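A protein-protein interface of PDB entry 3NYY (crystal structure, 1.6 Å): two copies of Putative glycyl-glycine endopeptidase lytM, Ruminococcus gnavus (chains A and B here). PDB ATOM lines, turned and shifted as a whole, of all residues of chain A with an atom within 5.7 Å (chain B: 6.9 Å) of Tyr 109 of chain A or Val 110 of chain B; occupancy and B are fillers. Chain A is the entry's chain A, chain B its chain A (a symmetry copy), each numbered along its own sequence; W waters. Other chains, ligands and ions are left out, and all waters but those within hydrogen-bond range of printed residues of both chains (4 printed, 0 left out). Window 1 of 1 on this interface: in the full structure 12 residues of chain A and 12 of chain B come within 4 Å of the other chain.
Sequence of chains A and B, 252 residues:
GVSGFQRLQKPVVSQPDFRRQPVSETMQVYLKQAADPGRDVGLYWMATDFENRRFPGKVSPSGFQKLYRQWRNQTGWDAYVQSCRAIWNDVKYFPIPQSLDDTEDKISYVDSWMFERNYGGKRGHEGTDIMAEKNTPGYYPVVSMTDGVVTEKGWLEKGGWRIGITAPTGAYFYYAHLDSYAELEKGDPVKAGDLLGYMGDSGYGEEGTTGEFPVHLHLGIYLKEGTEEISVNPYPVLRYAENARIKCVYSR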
ATOM      1  N   PHE A  94     -28.161   7.245 -17.830  1.00  0.00           N
ATOM      2  CA  PHE A  94     -27.826   7.723 -16.493  1.00  0.00           C
ATOM      3  C   PHE A  94     -26.546   6.955 -16.063  1.00  0.00           C
ATOM      4  O   PHE A  94     -26.320   5.829 -16.500  1.00  0.00           O
ATOM      5  CB  PHE A  94     -29.001   7.356 -15.587  1.00  0.00           C
ATOM      6  CG  PHE A  94     -28.983   8.047 -14.247  1.00  0.00           C
ATOM      7  CD1 PHE A  94     -29.340   9.382 -14.138  1.00  0.00           C
ATOM      8  CD2 PHE A  94     -28.665   7.339 -13.096  1.00  0.00           C
ATOM      9  CE1 PHE A  94     -29.317  10.013 -12.933  1.00  0.00           C
ATOM     10  CE2 PHE A  94     -28.641   7.969 -11.846  1.00  0.00           C
ATOM     11  CZ  PHE A  94     -28.942   9.305 -11.774  1.00  0.00           C
ATOM     12  N   ILE A 107     -30.476   5.829  -5.421  1.00  0.00           N
ATOM     13  CA  ILE A 107     -29.571   6.961  -5.293  1.00  0.00           C
ATOM     14  C   ILE A 107     -30.414   8.225  -5.139  1.00  0.00           C
ATOM     15  O   ILE A 107     -31.623   8.233  -5.412  1.00  0.00           O
ATOM     16  CB  ILE A 107     -28.583   7.102  -6.493  1.00  0.00           C
ATOM     17  CG1 ILE A 107     -29.280   6.995  -7.859  1.00  0.00           C
ATOM     18  CG2 ILE A 107     -27.479   6.024  -6.415  1.00  0.00           C
ATOM     19  CD1 ILE A 107     -30.190   8.155  -8.237  1.00  0.00           C
ATOM     20  N   SER A 108     -29.772   9.296  -4.714  1.00  0.00           N
ATOM     21  CA  SER A 108     -30.444  10.579  -4.499  1.00  0.00           C
ATOM     22  C   SER A 108     -29.499  11.663  -4.948  1.00  0.00           C
ATOM     23  O   SER A 108     -28.287  11.507  -4.803  1.00  0.00           O
ATOM     24  CB  SER A 108     -30.742  10.799  -3.016  1.00  0.00           C
ATOM     25  OG  SER A 108     -31.607   9.820  -2.492  1.00  0.00           O
ATOM     26  N   TYR A 109     -30.053  12.741  -5.513  1.00  0.00           N
ATOM     27  CA  TYR A 109     -29.254  13.864  -5.967  1.00  0.00           C
ATOM     28  C   TYR A 109     -30.127  15.090  -6.126  1.00  0.00           C
ATOM     29  O   TYR A 109     -31.340  14.978  -6.392  1.00  0.00           O
ATOM     30  CB  TYR A 109     -28.519  13.549  -7.264  1.00  0.00           C
ATOM     31  CG  TYR A 109     -29.391  13.301  -8.483  1.00  0.00           C
ATOM     32  CD1 TYR A 109     -29.998  12.084  -8.682  1.00  0.00           C
ATOM     33  CD2 TYR A 109     -29.555  14.297  -9.452  1.00  0.00           C
ATOM     34  CE1 TYR A 109     -30.794  11.849  -9.833  1.00  0.00           C
ATOM     35  CE2 TYR A 109     -30.339  14.070 -10.571  1.00  0.00           C
ATOM     36  CZ  TYR A 109     -30.924  12.860 -10.761  1.00  0.00           C
ATOM     37  OH  TYR A 109     -31.701  12.694 -11.897  1.00  0.00           O
ATOM     38  N   VAL A 110     -29.492  16.249  -5.972  1.00  0.00           N
ATOM     39  CA  VAL A 110     -30.149  17.547  -6.084  1.00  0.00           C
ATOM     40  C   VAL A 110     -29.334  18.457  -6.994  1.00  0.00           C
ATOM     41  O   VAL A 110     -28.184  18.163  -7.335  1.00  0.00           O
ATOM     42  CB  VAL A 110     -30.336  18.240  -4.711  1.00  0.00           C
ATOM     43  CG1 VAL A 110     -31.259  17.441  -3.783  1.00  0.00           C
ATOM     44  CG2 VAL A 110     -28.994  18.522  -4.049  1.00  0.00           C
ATOM     45  N   ASP A 111     -29.963  19.521  -7.440  1.00  0.00           N
ATOM     46  CA  ASP A 111     -29.295  20.595  -8.191  1.00  0.00           C
ATOM     47  C   ASP A 111     -28.563  21.481  -7.202  1.00  0.00           C
ATOM     48  O   ASP A 111     -29.162  22.351  -6.563  1.00  0.00           O
ATOM     49  CB  ASP A 111     -30.322  21.412  -8.958  1.00  0.00           C
ATOM     50  CG  ASP A 111     -29.693  22.343 -10.001  1.00  0.00           C
ATOM     51  OD1 ASP A 111     -28.481  22.567  -9.915  1.00  0.00           O
ATOM     52  OD2 ASP A 111     -30.444  22.818 -10.894  1.00  0.00           O
ATOM     53  N   THR A 128     -22.638  17.583 -10.031  1.00  0.00           N
ATOM     54  CA  THR A 128     -23.778  16.959  -9.344  1.00  0.00           C
ATOM     55  C   THR A 128     -23.240  15.758  -8.574  1.00  0.00           C
ATOM     56  O   THR A 128     -22.508  14.942  -9.090  1.00  0.00           O
ATOM     57  CB  THR A 128     -24.851  16.526 -10.303  1.00  0.00           C
ATOM     58  OG1 THR A 128     -25.286  17.668 -11.078  1.00  0.00           O
ATOM     59  CG2 THR A 128     -26.070  15.900  -9.560  1.00  0.00           C
ATOM     60  N   ASP A 129     -23.600  15.691  -7.300  1.00  0.00           N
ATOM     61  CA  ASP A 129     -23.239  14.585  -6.405  1.00  0.00           C
ATOM     62  C   ASP A 129     -24.363  13.585  -6.296  1.00  0.00           C
ATOM     63  O   ASP A 129     -25.445  13.896  -5.811  1.00  0.00           O
ATOM     64  CB  ASP A 129     -22.824  15.137  -5.053  1.00  0.00           C
ATOM     65  CG  ASP A 129     -21.568  15.987  -5.152  1.00  0.00           C
ATOM     66  OD1 ASP A 129     -20.679  15.600  -5.916  1.00  0.00           O
ATOM     67  OD2 ASP A 129     -21.513  17.075  -4.560  1.00  0.00           O
ATOM     68  N   ILE A 130     -24.127  12.388  -6.808  1.00  0.00           N
ATOM     69  CA  ILE A 130     -25.120  11.343  -6.824  1.00  0.00           C
ATOM     70  C   ILE A 130     -24.829  10.412  -5.620  1.00  0.00           C
ATOM     71  O   ILE A 130     -23.833   9.643  -5.599  1.00  0.00           O
ATOM     72  CB  ILE A 130     -25.123  10.626  -8.123  1.00  0.00           C
ATOM     73  CG1 ILE A 130     -25.482  11.579  -9.268  1.00  0.00           C
ATOM     74  CG2 ILE A 130     -26.130   9.476  -8.069  1.00  0.00           C
ATOM     75  CD1 ILE A 130     -25.210  10.986 -10.644  1.00  0.00           C
ATOM     76  N   MET A 131     -25.711  10.493  -4.625  1.00  0.00           N
ATOM     77  CA  MET A 131     -25.498   9.877  -3.326  1.00  0.00           C
ATOM     78  C   MET A 131     -25.994   8.470  -3.250  1.00  0.00           C
ATOM     79  O   MET A 131     -27.107   8.161  -3.685  1.00  0.00           O
ATOM     80  CB  MET A 131     -26.123  10.708  -2.193  1.00  0.00           C
ATOM     81  CG  MET A 131     -25.821  12.226  -2.247  1.00  0.00           C
ATOM     82  SD  MET A 131     -24.002  12.717  -2.003  1.00  0.00           S
ATOM     83  CE  MET A 131     -24.180  14.643  -1.686  1.00  0.00           C
ATOM     84  N   TYR A 235     -27.060  18.674 -13.668  1.00  0.00           N
ATOM     85  CA  TYR A 235     -28.307  18.236 -13.091  1.00  0.00           C
ATOM     86  C   TYR A 235     -29.436  18.051 -14.127  1.00  0.00           C
ATOM     87  O   TYR A 235     -30.072  16.989 -14.166  1.00  0.00           O
ATOM     88  CB  TYR A 235     -28.743  19.172 -11.937  1.00  0.00           C
ATOM     89  CG  TYR A 235     -30.086  18.813 -11.350  1.00  0.00           C
ATOM     90  CD1 TYR A 235     -30.156  17.831 -10.366  1.00  0.00           C
ATOM     91  CD2 TYR A 235     -31.281  19.411 -11.790  1.00  0.00           C
ATOM     92  CE1 TYR A 235     -31.357  17.462  -9.801  1.00  0.00           C
ATOM     93  CE2 TYR A 235     -32.515  19.010 -11.190  1.00  0.00           C
ATOM     94  CZ  TYR A 235     -32.509  18.017 -10.223  1.00  0.00           C
ATOM     95  OH  TYR A 235     -33.685  17.557  -9.585  1.00  0.00           O
ATOM     96  N   LEU A 238     -28.945  15.016 -16.269  1.00  0.00           N
ATOM     97  CA  LEU A 238     -29.119  13.823 -15.447  1.00  0.00           C
ATOM     98  C   LEU A 238     -30.589  13.523 -15.273  1.00  0.00           C
ATOM     99  O   LEU A 238     -30.977  12.361 -15.368  1.00  0.00           O
ATOM    100  CB  LEU A 238     -28.453  13.956 -14.079  1.00  0.00           C
ATOM    101  CG  LEU A 238     -26.946  13.792 -14.067  1.00  0.00           C
ATOM    102  CD1 LEU A 238     -26.310  14.307 -12.779  1.00  0.00           C
ATOM    103  CD2 LEU A 238     -26.519  12.273 -14.313  1.00  0.00           C
ATOM    104  N   ARG A 239     -31.408  14.561 -15.006  1.00  0.00           N
ATOM    105  CA  ARG A 239     -32.859  14.373 -14.876  1.00  0.00           C
ATOM    106  C   ARG A 239     -33.455  13.834 -16.145  1.00  0.00           C
ATOM    107  O   ARG A 239     -34.325  12.963 -16.117  1.00  0.00           O
ATOM    108  CB  ARG A 239     -33.559  15.677 -14.505  1.00  0.00           C
ATOM    109  CG  ARG A 239     -33.255  16.150 -13.112  1.00  0.00           C
ATOM    110  CD  ARG A 239     -33.742  15.215 -12.047  1.00  0.00           C
ATOM    111  NE  ARG A 239     -35.122  14.764 -12.206  1.00  0.00           N
ATOM    112  CZ  ARG A 239     -36.191  15.358 -11.694  1.00  0.00           C
ATOM    113  NH1 ARG A 239     -36.091  16.491 -10.987  1.00  0.00           N
ATOM    114  NH2 ARG A 239     -37.385  14.791 -11.872  1.00  0.00           N
ATOM    115  N   GLU A 242     -32.756  10.184 -16.336  1.00  0.00           N
ATOM    116  CA  GLU A 242     -33.144   9.485 -15.099  1.00  0.00           C
ATOM    117  C   GLU A 242     -33.765   8.117 -15.343  1.00  0.00           C
ATOM    118  O   GLU A 242     -33.447   7.158 -14.645  1.00  0.00           O
ATOM    119  CB  GLU A 242     -34.130  10.361 -14.279  1.00  0.00           C
ATOM    120  CG  GLU A 242     -35.524  10.551 -14.879  1.00  0.00           C
ATOM    121  CD  GLU A 242     -36.252  11.786 -14.340  1.00  0.00           C
ATOM    122  OE1 GLU A 242     -35.847  12.309 -13.267  1.00  0.00           O
ATOM    123  OE2 GLU A 242     -37.221  12.227 -15.017  1.00  0.00           O
ATOM    124  N   SER B 108     -36.762  16.717  -3.498  1.00  0.00           N
ATOM    125  CA  SER B 108     -35.523  15.936  -3.524  1.00  0.00           C
ATOM    126  C   SER B 108     -34.616  16.496  -2.459  1.00  0.00           C
ATOM    127  O   SER B 108     -34.647  17.701  -2.211  1.00  0.00           O
ATOM    128  CB  SER B 108     -34.813  16.082  -4.870  1.00  0.00           C
ATOM    129  OG  SER B 108     -35.591  15.602  -5.941  1.00  0.00           O
ATOM    130  N   TYR B 109     -33.836  15.619  -1.819  1.00  0.00           N
ATOM    131  CA  TYR B 109     -32.902  16.034  -0.789  1.00  0.00           C
ATOM    132  C   TYR B 109     -31.859  14.959  -0.572  1.00  0.00           C
ATOM    133  O   TYR B 109     -32.122  13.761  -0.798  1.00  0.00           O
ATOM    134  CB  TYR B 109     -33.612  16.371   0.517  1.00  0.00           C
ATOM    135  CG  TYR B 109     -34.318  15.219   1.211  1.00  0.00           C
ATOM    136  CD1 TYR B 109     -35.558  14.796   0.795  1.00  0.00           C
ATOM    137  CD2 TYR B 109     -33.735  14.594   2.319  1.00  0.00           C
ATOM    138  CE1 TYR B 109     -36.224  13.734   1.459  1.00  0.00           C
ATOM    139  CE2 TYR B 109     -34.381  13.551   2.962  1.00  0.00           C
ATOM    140  CZ  TYR B 109     -35.611  13.152   2.549  1.00  0.00           C
ATOM    141  OH  TYR B 109     -36.206  12.099   3.229  1.00  0.00           O
ATOM    142  N   VAL B 110     -30.686  15.403  -0.126  1.00  0.00           N
ATOM    143  CA  VAL B 110     -29.548  14.534   0.147  1.00  0.00           C
ATOM    144  C   VAL B 110     -28.972  14.858   1.520  1.00  0.00           C
ATOM    145  O   VAL B 110     -29.305  15.877   2.132  1.00  0.00           O
ATOM    146  CB  VAL B 110     -28.429  14.668  -0.916  1.00  0.00           C
ATOM    147  CG1 VAL B 110     -28.899  14.230  -2.308  1.00  0.00           C
ATOM    148  CG2 VAL B 110     -27.860  16.080  -0.943  1.00  0.00           C
ATOM    149  N   ASP B 111     -28.167  13.949   2.024  1.00  0.00           N
ATOM    150  CA  ASP B 111     -27.391  14.157   3.255  1.00  0.00           C
ATOM    151  C   ASP B 111     -26.176  14.999   2.914  1.00  0.00           C
ATOM    152  O   ASP B 111     -25.170  14.489   2.410  1.00  0.00           O
ATOM    153  CB  ASP B 111     -26.950  12.820   3.827  1.00  0.00           C
ATOM    154  CG  ASP B 111     -26.412  12.925   5.258  1.00  0.00           C
ATOM    155  OD1 ASP B 111     -26.107  14.046   5.677  1.00  0.00           O
ATOM    156  OD2 ASP B 111     -26.321  11.864   5.932  1.00  0.00           O
ATOM    157  N   SER B 112     -26.248  16.278   3.225  1.00  0.00           N
ATOM    158  CA  SER B 112     -25.153  17.211   2.900  1.00  0.00           C
ATOM    159  C   SER B 112     -24.243  17.514   4.078  1.00  0.00           C
ATOM    160  O   SER B 112     -23.362  18.375   3.977  1.00  0.00           O
ATOM    161  CB  SER B 112     -25.762  18.511   2.373  1.00  0.00           C
ATOM    162  OG  SER B 112     -26.652  19.066   3.332  1.00  0.00           O
ATOM    163  N   TRP B 113     -24.451  16.827   5.199  1.00  0.00           N
ATOM    164  CA  TRP B 113     -23.800  17.148   6.454  1.00  0.00           C
ATOM    165  C   TRP B 113     -22.276  17.191   6.336  1.00  0.00           C
ATOM    166  O   TRP B 113     -21.643  18.146   6.758  1.00  0.00           O
ATOM    167  CB  TRP B 113     -24.215  16.146   7.550  1.00  0.00           C
ATOM    168  CG  TRP B 113     -23.749  16.610   8.900  1.00  0.00           C
ATOM    169  CD1 TRP B 113     -22.669  16.177   9.604  1.00  0.00           C
ATOM    170  CD2 TRP B 113     -24.340  17.656   9.644  1.00  0.00           C
ATOM    171  NE1 TRP B 113     -22.578  16.889  10.794  1.00  0.00           N
ATOM    172  CE2 TRP B 113     -23.608  17.787  10.840  1.00  0.00           C
ATOM    173  CE3 TRP B 113     -25.466  18.470   9.447  1.00  0.00           C
ATOM    174  CZ2 TRP B 113     -23.920  18.751  11.790  1.00  0.00           C
ATOM    175  CZ3 TRP B 113     -25.793  19.407  10.407  1.00  0.00           C
ATOM    176  CH2 TRP B 113     -25.008  19.551  11.552  1.00  0.00           C
ATOM    177  N   PHE B 115     -20.433  17.449   3.666  1.00  0.00           N
ATOM    178  CA  PHE B 115     -20.035  18.433   2.677  1.00  0.00           C
ATOM    179  C   PHE B 115     -20.046  19.818   3.392  1.00  0.00           C
ATOM    180  O   PHE B 115     -19.085  20.579   3.307  1.00  0.00           O
ATOM    181  CB  PHE B 115     -20.971  18.340   1.447  1.00  0.00           C
ATOM    182  CG  PHE B 115     -20.946  16.965   0.760  1.00  0.00           C
ATOM    183  CD1 PHE B 115     -21.603  15.856   1.323  1.00  0.00           C
ATOM    184  CD2 PHE B 115     -20.232  16.771  -0.421  1.00  0.00           C
ATOM    185  CE1 PHE B 115     -21.549  14.578   0.716  1.00  0.00           C
ATOM    186  CE2 PHE B 115     -20.190  15.505  -1.045  1.00  0.00           C
ATOM    187  CZ  PHE B 115     -20.832  14.409  -0.472  1.00  0.00           C
ATOM    188  N   GLU B 116     -21.099  20.098   4.166  1.00  0.00           N
ATOM    189  CA  GLU B 116     -21.260  21.393   4.874  1.00  0.00           C
ATOM    190  C   GLU B 116     -20.283  21.630   6.026  1.00  0.00           C
ATOM    191  O   GLU B 116     -19.835  22.769   6.227  1.00  0.00           O
ATOM    192  CB  GLU B 116     -22.699  21.535   5.423  1.00  0.00           C
ATOM    193  CG  GLU B 116     -23.725  21.809   4.329  1.00  0.00           C
ATOM    194  CD  GLU B 116     -25.174  21.587   4.763  1.00  0.00           C
ATOM    195  OE1 GLU B 116     -25.464  21.504   5.978  1.00  0.00           O
ATOM    196  OE2 GLU B 116     -26.033  21.484   3.862  1.00  0.00           O
ATOM    197  N   GLY B 127     -27.710  21.918   7.822  1.00  0.00           N
ATOM    198  CA  GLY B 127     -28.999  21.222   7.932  1.00  0.00           C
ATOM    199  C   GLY B 127     -29.244  20.368   6.714  1.00  0.00           C
ATOM    200  O   GLY B 127     -28.286  19.752   6.206  1.00  0.00           O
ATOM    201  N   THR B 128     -30.495  20.323   6.278  1.00  0.00           N
ATOM    202  CA  THR B 128     -30.899  19.576   5.076  1.00  0.00           C
ATOM    203  C   THR B 128     -31.723  20.524   4.211  1.00  0.00           C
ATOM    204  O   THR B 128     -32.628  21.186   4.671  1.00  0.00           O
ATOM    205  CB  THR B 128     -31.697  18.348   5.414  1.00  0.00           C
ATOM    206  OG1 THR B 128     -30.924  17.507   6.301  1.00  0.00           O
ATOM    207  CG2 THR B 128     -32.087  17.546   4.135  1.00  0.00           C
ATOM    208  N   ASP B 129     -31.358  20.594   2.939  1.00  0.00           N
ATOM    209  CA  ASP B 129     -32.059  21.399   1.931  1.00  0.00           C
ATOM    210  C   ASP B 129     -33.016  20.551   1.129  1.00  0.00           C
ATOM    211  O   ASP B 129     -32.614  19.638   0.419  1.00  0.00           O
ATOM    212  CB  ASP B 129     -31.047  22.113   1.054  1.00  0.00           C
ATOM    213  CG  ASP B 129     -30.220  23.112   1.846  1.00  0.00           C
ATOM    214  OD1 ASP B 129     -30.802  23.772   2.713  1.00  0.00           O
ATOM    215  OD2 ASP B 129     -28.992  23.162   1.681  1.00  0.00           O
ATOM    216  N   ILE B 130     -34.303  20.817   1.292  1.00  0.00           N
ATOM    217  CA  ILE B 130     -35.338  20.061   0.633  1.00  0.00           C
ATOM    218  C   ILE B 130     -35.772  20.866  -0.618  1.00  0.00           C
ATOM    219  O   ILE B 130     -36.429  21.935  -0.527  1.00  0.00           O
ATOM    220  CB  ILE B 130     -36.464  19.777   1.557  1.00  0.00           C
ATOM    221  CG1 ILE B 130     -35.994  18.922   2.739  1.00  0.00           C
ATOM    222  CG2 ILE B 130     -37.574  19.047   0.798  1.00  0.00           C
ATOM    223  CD1 ILE B 130     -37.015  18.850   3.865  1.00  0.00           C
ATOM    224  N   MET B 131     -35.394  20.338  -1.781  1.00  0.00           N
ATOM    225  CA  MET B 131     -35.503  21.045  -3.046  1.00  0.00           C
ATOM    226  C   MET B 131     -36.819  20.844  -3.724  1.00  0.00           C
ATOM    227  O   MET B 131     -37.320  19.721  -3.826  1.00  0.00           O
ATOM    228  CB  MET B 131     -34.362  20.672  -4.007  1.00  0.00           C
ATOM    229  CG  MET B 131     -32.946  20.679  -3.381  1.00  0.00           C
ATOM    230  SD  MET B 131     -32.304  22.373  -2.806  1.00  0.00           S
ATOM    231  CE  MET B 131     -30.401  21.977  -2.549  1.00  0.00           C
ATOM    232  N   ASN B 233     -27.553  16.862  12.282  1.00  0.00           N
ATOM    233  CA  ASN B 233     -27.998  16.458  10.952  1.00  0.00           C
ATOM    234  C   ASN B 233     -29.463  16.048  10.932  1.00  0.00           C
ATOM    235  O   ASN B 233     -29.814  15.021  11.538  1.00  0.00           O
ATOM    236  CB  ASN B 233     -27.113  15.311  10.462  1.00  0.00           C
ATOM    237  CG  ASN B 233     -27.280  14.996   8.993  1.00  0.00           C
ATOM    238  OD1 ASN B 233     -27.984  15.719   8.246  1.00  0.00           O
ATOM    239  ND2 ASN B 233     -26.548  13.930   8.527  1.00  0.00           N
ATOM    240  N   TYR B 235     -30.986  14.871   8.279  1.00  0.00           N
ATOM    241  CA  TYR B 235     -31.260  13.959   7.196  1.00  0.00           C
ATOM    242  C   TYR B 235     -31.857  12.613   7.658  1.00  0.00           C
ATOM    243  O   TYR B 235     -32.898  12.186   7.140  1.00  0.00           O
ATOM    244  CB  TYR B 235     -30.004  13.750   6.316  1.00  0.00           C
ATOM    245  CG  TYR B 235     -30.206  12.739   5.214  1.00  0.00           C
ATOM    246  CD1 TYR B 235     -30.783  13.147   4.015  1.00  0.00           C
ATOM    247  CD2 TYR B 235     -29.865  11.383   5.370  1.00  0.00           C
ATOM    248  CE1 TYR B 235     -30.994  12.262   2.980  1.00  0.00           C
ATOM    249  CE2 TYR B 235     -30.096  10.483   4.283  1.00  0.00           C
ATOM    250  CZ  TYR B 235     -30.685  10.959   3.122  1.00  0.00           C
ATOM    251  OH  TYR B 235     -30.954  10.136   2.003  1.00  0.00           O
HETATM  252  O   HOH W   1     -33.412  15.501  -7.864  1.00  0.00           O
HETATM  253  O   HOH W   2     -24.408  12.097   1.243  1.00  0.00           O
HETATM  254  O   HOH W   3     -31.767  23.109  -6.009  1.00  0.00           O
HETATM  255  O   HOH W   4     -32.259  11.277  -0.061  1.00  0.00           O
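The backbone NH of Met 131 of chain A lies within hydrogen-bond range of the backbone carbonyl oxygen of Ser 108 of chain A (2.8 Å). The backbone carbonyl oxygen (O) of Ser 108 of chain B is in hydrogen-bond range of the backbone NH (N) of Met 131 of chain B (2.8 Å).
Among the printed residues, pairs that only touch across the chains: Met 131 of chain A with Phe 115 of chain B, Val 110 of chain A with Met 131 of chain B, Met 131 of chain A with Val 110 of chain B, Val 110 of chain A with Tyr 109 of chain B, Tyr 109 of chain A with Val 110 of chain B, Val 110 of chain A with Ser 108 of chain B, Ser 108 of chain A with Val 110 of chain B, Tyr 109 of chain A with Ser 108 of chain B and Ser 108 of chain A with Tyr 109 of chain B.
Of the printed residues of chain B, Tyr 109 of chain A touches Ser 108 (3.9 Å) and Val 110 (3.7 Å). Of the printed residues of chain B, Val 110 of chain A touches Ser 108, Tyr 109 and Met 131. Printed residues of chain B within 4 Å of Met 131 of chain A: Val 110 and Phe 115. Printed residues of chain A within 4 Å of Ser 108 of chain B: Tyr 109 (3.9 Å) and Val 110 (3.7 Å). Of the printed residues of chain A, Val 110 of chain B touches Ser 108 (3.7 Å), Tyr 109 (3.7 Å) and Met 131 (3.7 Å). Printed residues of chain A within 4 Å of Phe 115 of chain B: Met 131 (3.6 Å). Of the printed residues of chain A, Met 131 of chain B touches Val 110. The nearest printed residue of chain B that does not touch Tyr 109 of chain A is Tyr 109 of chain B (5.2 Å). The nearest printed residue of chain A that does not touch Ser 108 of chain B is Tyr 235 of chain A (4.6 Å).
Printed residues of chain B that touch a printed residue of chain A: Ser 108, Tyr 109, Val 110, Phe 115 and Met 131. Of the 14 printed residues of chain A, 4 touch a printed residue of chain B. Hydrophobic or aromatic side chains of chain A within 4 Å of the printed part of chain B: Val 110 and Met 131.
Ser 108 of chain A touches Tyr 109 of chain B, and with the chains exchanged Tyr 109 of chain A touches Ser 108 of chain B. Ser 108 of chain A touches Val 110 of chain B, and with the chains exchanged Val 110 of chain A touches Ser 108 of chain B. Tyr 109 of chain A touches Val 110 of chain B, and with the chains exchanged Val 110 of chain A touches Tyr 109 of chain B. Val 110 of chain A touches Met 131 of chain B, and with the chains exchanged Met 131 of chain A touches Val 110 of chain B. Positions printed for both chains: 108, 109, 110, 111, 128, 129, 130, 131 and 235. Of the 9 pairs that touch across the chains among the printed residues, 8 have their exchanged pair printed and touching as well.
Water W1 lies within hydrogen-bond range of O of Tyr 109 of chain A (2.6 Å), OH of Tyr 235 of chain A (2.7 Å) and OG of Ser 108 of chain B (2.9 Å). Water W4 lies within hydrogen-bond range of O of Tyr 109 of chain B, OH of Tyr 235 of chain B and OG of Ser 108 of chain A. Water W3 bridges O of Asp 111 of chain A (2.8 Å) and SD of Met 131 of chain B (3.3 Å). Water W2 bridges O of Asp 111 of chain B (2.8 Å) and SD of Met 131 of chain A (3.3 Å).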
